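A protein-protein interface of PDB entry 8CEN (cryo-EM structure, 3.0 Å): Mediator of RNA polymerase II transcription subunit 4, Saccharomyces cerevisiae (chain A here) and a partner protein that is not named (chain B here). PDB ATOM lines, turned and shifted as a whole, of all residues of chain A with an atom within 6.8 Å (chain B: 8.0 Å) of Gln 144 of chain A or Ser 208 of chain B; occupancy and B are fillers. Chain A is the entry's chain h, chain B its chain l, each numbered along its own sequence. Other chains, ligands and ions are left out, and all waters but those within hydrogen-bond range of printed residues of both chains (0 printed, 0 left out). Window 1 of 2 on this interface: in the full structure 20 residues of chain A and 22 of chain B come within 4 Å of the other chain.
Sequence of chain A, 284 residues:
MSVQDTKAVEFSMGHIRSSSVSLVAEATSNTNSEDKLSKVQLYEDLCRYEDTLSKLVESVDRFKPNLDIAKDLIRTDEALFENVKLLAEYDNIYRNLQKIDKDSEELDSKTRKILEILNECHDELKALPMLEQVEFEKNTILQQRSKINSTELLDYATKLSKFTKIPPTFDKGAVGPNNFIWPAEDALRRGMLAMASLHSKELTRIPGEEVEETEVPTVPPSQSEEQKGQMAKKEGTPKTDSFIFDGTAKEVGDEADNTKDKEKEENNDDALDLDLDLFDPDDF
OG of Ser 208 of chain B sits at hydrogen-bond distance from NE2 of Gln 144 of chain A.
O of Leu 204 of chain B is in hydrogen-bond range of OG of Ser 208 of chain B (2.7 Å).
Lys 147 of chain A touches Leu 207 of chain B.
Ile 148 of chain A touches Leu 204 of chain B (CD1 to CD2, 3.7 Å).
Ile 148 of chain A touches Leu 207 of chain B (CD1 to CB, 3.6 Å).
Ser 208 of chain B touches Ile 148 of chain A (OG to CD1, 3.8 Å).
Gln 144 of chain A touches one residue of chain B.
Ser 208 of chain B touches just these residues of chain A: Gln 144 (2.4 Å) and Ile 148 (3.8 Å).
Of the printed residues of chain B, Ile 148 of chain A touches Leu 204, Leu 207 and Ser 208.
Printed residues of chain B within 4 Å of Lys 147 of chain A: Leu 207.
Of the printed residues of chain A, Leu 207 of chain B touches Lys 147 and Ile 148.
Arg 211 of chain B touches none of the printed residues of chain A.
Ser 146 of chain A touches none of the printed residues of chain B.
The nearest residue of chain A that does not touch Ser 208 of chain B is Lys 147 of chain A (4.5 Å).
The nearest printed residue of chain A that does not touch Leu 207 of chain B is Asn 149 of chain A (5.0 Å).
Printed residues of chain B that touch a printed residue of chain A: Leu 204, Leu 207 and Ser 208.
Among the printed residues, 5 pairs touch across the chains.
Among the printed residues, no Asp or Glu carboxylate lies within 4 Å of a Lys or Arg side-chain nitrogen of the other chain.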
ATOM      1  N   ASN A 139     -37.209  17.727 -34.996  1.00  0.00           N
ATOM      2  CA  ASN A 139     -37.814  16.515 -34.456  1.00  0.00           C
ATOM      3  C   ASN A 139     -36.758  15.561 -33.914  1.00  0.00           C
ATOM      4  O   ASN A 139     -36.967  14.924 -32.878  1.00  0.00           O
ATOM      5  CB  ASN A 139     -38.661  15.828 -35.527  1.00  0.00           C
ATOM      6  CG  ASN A 139     -39.916  16.607 -35.864  1.00  0.00           C
ATOM      7  OD1 ASN A 139     -40.587  17.138 -34.979  1.00  0.00           O
ATOM      8  ND2 ASN A 139     -40.239  16.684 -37.150  1.00  0.00           N
ATOM      9  N   THR A 140     -35.612  15.460 -34.593  1.00  0.00           N
ATOM     10  CA  THR A 140     -34.520  14.628 -34.098  1.00  0.00           C
ATOM     11  C   THR A 140     -33.957  15.174 -32.789  1.00  0.00           C
ATOM     12  O   THR A 140     -33.662  14.407 -31.860  1.00  0.00           O
ATOM     13  CB  THR A 140     -33.424  14.527 -35.158  1.00  0.00           C
ATOM     14  OG1 THR A 140     -33.998  14.092 -36.396  1.00  0.00           O
ATOM     15  CG2 THR A 140     -32.367  13.526 -34.740  1.00  0.00           C
ATOM     16  N   ILE A 141     -33.817  16.500 -32.694  1.00  0.00           N
ATOM     17  CA  ILE A 141     -33.328  17.129 -31.467  1.00  0.00           C
ATOM     18  C   ILE A 141     -34.292  16.874 -30.312  1.00  0.00           C
ATOM     19  O   ILE A 141     -33.873  16.535 -29.197  1.00  0.00           O
ATOM     20  CB  ILE A 141     -33.094  18.634 -31.703  1.00  0.00           C
ATOM     21  CG1 ILE A 141     -31.845  18.849 -32.562  1.00  0.00           C
ATOM     22  CG2 ILE A 141     -32.969  19.389 -30.384  1.00  0.00           C
ATOM     23  CD1 ILE A 141     -31.448  20.302 -32.728  1.00  0.00           C
ATOM     24  N   LEU A 142     -35.596  17.003 -30.566  1.00  0.00           N
ATOM     25  CA  LEU A 142     -36.581  16.737 -29.520  1.00  0.00           C
ATOM     26  C   LEU A 142     -36.680  15.250 -29.185  1.00  0.00           C
ATOM     27  O   LEU A 142     -37.053  14.897 -28.061  1.00  0.00           O
ATOM     28  CB  LEU A 142     -37.952  17.284 -29.920  1.00  0.00           C
ATOM     29  CG  LEU A 142     -38.316  18.728 -29.543  1.00  0.00           C
ATOM     30  CD1 LEU A 142     -38.362  18.873 -28.029  1.00  0.00           C
ATOM     31  CD2 LEU A 142     -37.384  19.770 -30.149  1.00  0.00           C
ATOM     32  N   GLN A 143     -36.366  14.365 -30.135  1.00  0.00           N
ATOM     33  CA  GLN A 143     -36.354  12.938 -29.835  1.00  0.00           C
ATOM     34  C   GLN A 143     -35.131  12.535 -29.023  1.00  0.00           C
ATOM     35  O   GLN A 143     -35.187  11.551 -28.278  1.00  0.00           O
ATOM     36  CB  GLN A 143     -36.420  12.116 -31.128  1.00  0.00           C
ATOM     37  CG  GLN A 143     -37.805  11.969 -31.815  1.00  0.00           C
ATOM     38  CD  GLN A 143     -38.888  11.206 -31.028  1.00  0.00           C
ATOM     39  OE1 GLN A 143     -38.962  11.239 -29.799  1.00  0.00           O
ATOM     40  NE2 GLN A 143     -39.740  10.508 -31.768  1.00  0.00           N
ATOM     41  N   GLN A 144     -34.023  13.271 -29.159  1.00  0.00           N
ATOM     42  CA  GLN A 144     -32.872  13.038 -28.289  1.00  0.00           C
ATOM     43  C   GLN A 144     -33.159  13.378 -26.831  1.00  0.00           C
ATOM     44  O   GLN A 144     -32.451  12.883 -25.947  1.00  0.00           O
ATOM     45  CB  GLN A 144     -31.661  13.840 -28.766  1.00  0.00           C
ATOM     46  CG  GLN A 144     -31.123  13.424 -30.118  1.00  0.00           C
ATOM     47  CD  GLN A 144     -30.615  12.001 -30.126  1.00  0.00           C
ATOM     48  OE1 GLN A 144     -31.221  11.115 -30.727  1.00  0.00           O
ATOM     49  NE2 GLN A 144     -29.493  11.773 -29.455  1.00  0.00           N
ATOM     50  N   ARG A 145     -34.171  14.212 -26.569  1.00  0.00           N
ATOM     51  CA  ARG A 145     -34.517  14.587 -25.199  1.00  0.00           C
ATOM     52  C   ARG A 145     -34.976  13.384 -24.384  1.00  0.00           C
ATOM     53  O   ARG A 145     -34.579  13.222 -23.225  1.00  0.00           O
ATOM     54  CB  ARG A 145     -35.606  15.661 -25.218  1.00  0.00           C
ATOM     55  CG  ARG A 145     -36.070  16.128 -23.850  1.00  0.00           C
ATOM     56  CD  ARG A 145     -35.087  17.106 -23.231  1.00  0.00           C
ATOM     57  NE  ARG A 145     -35.064  18.379 -23.941  1.00  0.00           N
ATOM     58  CZ  ARG A 145     -35.967  19.340 -23.798  1.00  0.00           C
ATOM     59  NH1 ARG A 145     -36.983  19.217 -22.959  1.00  0.00           N
ATOM     60  NH2 ARG A 145     -35.845  20.455 -24.511  1.00  0.00           N
ATOM     61  N   SER A 146     -35.809  12.525 -24.976  1.00  0.00           N
ATOM     62  CA  SER A 146     -36.336  11.382 -24.238  1.00  0.00           C
ATOM     63  C   SER A 146     -35.289  10.291 -24.053  1.00  0.00           C
ATOM     64  O   SER A 146     -35.327   9.563 -23.055  1.00  0.00           O
ATOM     65  CB  SER A 146     -37.566  10.819 -24.950  1.00  0.00           C
ATOM     66  OG  SER A 146     -37.202  10.155 -26.146  1.00  0.00           O
ATOM     67  N   LYS A 147     -34.352  10.162 -24.992  1.00  0.00           N
ATOM     68  CA  LYS A 147     -33.367   9.088 -24.938  1.00  0.00           C
ATOM     69  C   LYS A 147     -32.104   9.457 -24.174  1.00  0.00           C
ATOM     70  O   LYS A 147     -31.440   8.564 -23.635  1.00  0.00           O
ATOM     71  CB  LYS A 147     -32.983   8.648 -26.354  1.00  0.00           C
ATOM     72  CG  LYS A 147     -34.102   7.961 -27.116  1.00  0.00           C
ATOM     73  CD  LYS A 147     -33.965   6.448 -27.022  1.00  0.00           C
ATOM     74  CE  LYS A 147     -34.916   5.741 -27.971  1.00  0.00           C
ATOM     75  NZ  LYS A 147     -34.393   4.408 -28.382  1.00  0.00           N
ATOM     76  N   ILE A 148     -31.745  10.735 -24.111  1.00  0.00           N
ATOM     77  CA  ILE A 148     -30.446  11.150 -23.598  1.00  0.00           C
ATOM     78  C   ILE A 148     -30.642  11.782 -22.226  1.00  0.00           C
ATOM     79  O   ILE A 148     -31.412  12.739 -22.076  1.00  0.00           O
ATOM     80  CB  ILE A 148     -29.755  12.123 -24.565  1.00  0.00           C
ATOM     81  CG1 ILE A 148     -29.223  11.368 -25.785  1.00  0.00           C
ATOM     82  CG2 ILE A 148     -28.609  12.833 -23.874  1.00  0.00           C
ATOM     83  CD1 ILE A 148     -27.967  10.579 -25.535  1.00  0.00           C
ATOM     84  N   ASN A 149     -29.952  11.245 -21.224  1.00  0.00           N
ATOM     85  CA  ASN A 149     -29.932  11.787 -19.873  1.00  0.00           C
ATOM     86  C   ASN A 149     -28.516  12.254 -19.561  1.00  0.00           C
ATOM     87  O   ASN A 149     -27.545  11.609 -19.964  1.00  0.00           O
ATOM     88  CB  ASN A 149     -30.386  10.732 -18.857  1.00  0.00           C
ATOM     89  CG  ASN A 149     -30.636  11.309 -17.474  1.00  0.00           C
ATOM     90  OD1 ASN A 149     -30.482  12.507 -17.243  1.00  0.00           O
ATOM     91  ND2 ASN A 149     -31.026  10.447 -16.542  1.00  0.00           N
ATOM     92  N   LEU B 200     -17.652  11.539 -25.003  1.00  0.00           N
ATOM     93  CA  LEU B 200     -19.015  11.982 -25.249  1.00  0.00           C
ATOM     94  C   LEU B 200     -19.510  11.521 -26.610  1.00  0.00           C
ATOM     95  O   LEU B 200     -20.706  11.276 -26.768  1.00  0.00           O
ATOM     96  CB  LEU B 200     -19.100  13.503 -25.141  1.00  0.00           C
ATOM     97  CG  LEU B 200     -18.591  14.110 -23.834  1.00  0.00           C
ATOM     98  CD1 LEU B 200     -18.355  15.596 -24.006  1.00  0.00           C
ATOM     99  CD2 LEU B 200     -19.571  13.848 -22.704  1.00  0.00           C
ATOM    100  N   VAL B 201     -18.611  11.384 -27.588  1.00  0.00           N
ATOM    101  CA  VAL B 201     -19.015  10.972 -28.932  1.00  0.00           C
ATOM    102  C   VAL B 201     -19.582   9.557 -28.904  1.00  0.00           C
ATOM    103  O   VAL B 201     -20.698   9.301 -29.380  1.00  0.00           O
ATOM    104  CB  VAL B 201     -17.820  11.075 -29.899  1.00  0.00           C
ATOM    105  CG1 VAL B 201     -18.151  10.427 -31.234  1.00  0.00           C
ATOM    106  CG2 VAL B 201     -17.388  12.522 -30.076  1.00  0.00           C
ATOM    107  N   THR B 202     -18.834   8.627 -28.305  1.00  0.00           N
ATOM    108  CA  THR B 202     -19.296   7.248 -28.205  1.00  0.00           C
ATOM    109  C   THR B 202     -20.498   7.136 -27.278  1.00  0.00           C
ATOM    110  O   THR B 202     -21.415   6.346 -27.543  1.00  0.00           O
ATOM    111  CB  THR B 202     -18.155   6.345 -27.738  1.00  0.00           C
ATOM    112  OG1 THR B 202     -16.967   6.665 -28.470  1.00  0.00           O
ATOM    113  CG2 THR B 202     -18.495   4.882 -27.981  1.00  0.00           C
ATOM    114  N   ALA B 203     -20.527   7.936 -26.202  1.00  0.00           N
ATOM    115  CA  ALA B 203     -21.688   7.923 -25.315  1.00  0.00           C
ATOM    116  C   ALA B 203     -22.959   8.353 -26.041  1.00  0.00           C
ATOM    117  O   ALA B 203     -24.004   7.707 -25.901  1.00  0.00           O
ATOM    118  CB  ALA B 203     -21.439   8.824 -24.109  1.00  0.00           C
ATOM    119  N   LEU B 204     -22.885   9.426 -26.836  1.00  0.00           N
ATOM    120  CA  LEU B 204     -24.040   9.871 -27.610  1.00  0.00           C
ATOM    121  C   LEU B 204     -24.455   8.859 -28.665  1.00  0.00           C
ATOM    122  O   LEU B 204     -25.654   8.618 -28.840  1.00  0.00           O
ATOM    123  CB  LEU B 204     -23.770  11.230 -28.251  1.00  0.00           C
ATOM    124  CG  LEU B 204     -23.662  12.368 -27.249  1.00  0.00           C
ATOM    125  CD1 LEU B 204     -23.242  13.648 -27.910  1.00  0.00           C
ATOM    126  CD2 LEU B 204     -25.043  12.525 -26.695  1.00  0.00           C
ATOM    127  N   GLU B 205     -23.492   8.255 -29.374  1.00  0.00           N
ATOM    128  CA  GLU B 205     -23.856   7.260 -30.383  1.00  0.00           C
ATOM    129  C   GLU B 205     -24.583   6.077 -29.756  1.00  0.00           C
ATOM    130  O   GLU B 205     -25.646   5.662 -30.239  1.00  0.00           O
ATOM    131  CB  GLU B 205     -22.622   6.776 -31.148  1.00  0.00           C
ATOM    132  CG  GLU B 205     -21.920   7.832 -31.978  1.00  0.00           C
ATOM    133  CD  GLU B 205     -20.441   7.547 -32.148  1.00  0.00           C
ATOM    134  OE1 GLU B 205     -19.907   6.703 -31.401  1.00  0.00           O
ATOM    135  OE2 GLU B 205     -19.813   8.165 -33.034  1.00  0.00           O
ATOM    136  N   VAL B 206     -24.055   5.556 -28.646  1.00  0.00           N
ATOM    137  CA  VAL B 206     -24.649   4.371 -28.035  1.00  0.00           C
ATOM    138  C   VAL B 206     -25.986   4.702 -27.380  1.00  0.00           C
ATOM    139  O   VAL B 206     -26.952   3.941 -27.497  1.00  0.00           O
ATOM    140  CB  VAL B 206     -23.659   3.740 -27.044  1.00  0.00           C
ATOM    141  CG1 VAL B 206     -24.291   2.565 -26.335  1.00  0.00           C
ATOM    142  CG2 VAL B 206     -22.431   3.296 -27.782  1.00  0.00           C
ATOM    143  N   LEU B 207     -26.085   5.843 -26.700  1.00  0.00           N
ATOM    144  CA  LEU B 207     -27.340   6.163 -26.038  1.00  0.00           C
ATOM    145  C   LEU B 207     -28.384   6.743 -26.983  1.00  0.00           C
ATOM    146  O   LEU B 207     -29.540   6.898 -26.575  1.00  0.00           O
ATOM    147  CB  LEU B 207     -27.090   7.127 -24.879  1.00  0.00           C
ATOM    148  CG  LEU B 207     -26.238   6.599 -23.723  1.00  0.00           C
ATOM    149  CD1 LEU B 207     -26.203   7.601 -22.582  1.00  0.00           C
ATOM    150  CD2 LEU B 207     -26.749   5.251 -23.252  1.00  0.00           C
ATOM    151  N   SER B 208     -28.018   7.068 -28.225  1.00  0.00           N
ATOM    152  CA  SER B 208     -28.984   7.516 -29.220  1.00  0.00           C
ATOM    153  C   SER B 208     -29.453   6.376 -30.117  1.00  0.00           C
ATOM    154  O   SER B 208     -30.648   6.070 -30.162  1.00  0.00           O
ATOM    155  CB  SER B 208     -28.375   8.640 -30.066  1.00  0.00           C
ATOM    156  OG  SER B 208     -28.098   9.781 -29.272  1.00  0.00           O
ATOM    157  N   LEU B 209     -28.530   5.737 -30.836  1.00  0.00           N
ATOM    158  CA  LEU B 209     -28.905   4.717 -31.806  1.00  0.00           C
ATOM    159  C   LEU B 209     -28.834   3.300 -31.259  1.00  0.00           C
ATOM    160  O   LEU B 209     -29.268   2.368 -31.945  1.00  0.00           O
ATOM    161  CB  LEU B 209     -28.013   4.807 -33.049  1.00  0.00           C
ATOM    162  CG  LEU B 209     -27.764   6.173 -33.682  1.00  0.00           C
ATOM    163  CD1 LEU B 209     -26.833   6.014 -34.872  1.00  0.00           C
ATOM    164  CD2 LEU B 209     -29.071   6.822 -34.101  1.00  0.00           C
ATOM    165  N   GLY B 210     -28.303   3.109 -30.055  1.00  0.00           N
ATOM    166  CA  GLY B 210     -28.005   1.778 -29.580  1.00  0.00           C
ATOM    167  C   GLY B 210     -26.751   1.176 -30.166  1.00  0.00           C
ATOM    168  O   GLY B 210     -26.466   0.000 -29.908  1.00  0.00           O
ATOM    169  N   ARG B 211     -25.993   1.946 -30.940  1.00  0.00           N
ATOM    170  CA  ARG B 211     -24.829   1.473 -31.666  1.00  0.00           C
ATOM    171  C   ARG B 211     -23.836   2.618 -31.765  1.00  0.00           C
ATOM    172  O   ARG B 211     -24.243   3.783 -31.851  1.00  0.00           O
ATOM    173  CB  ARG B 211     -25.216   0.963 -33.069  1.00  0.00           C
ATOM    174  CG  ARG B 211     -25.702   2.070 -34.003  1.00  0.00           C
ATOM    175  CD  ARG B 211     -26.208   1.618 -35.356  1.00  0.00           C
ATOM    176  NE  ARG B 211     -26.461   2.792 -36.186  1.00  0.00           N
ATOM    177  CZ  ARG B 211     -27.059   2.777 -37.369  1.00  0.00           C
ATOM    178  NH1 ARG B 211     -27.504   1.655 -37.907  1.00  0.00           N
ATOM    179  NH2 ARG B 211     -27.223   3.921 -38.026  1.00  0.00           N
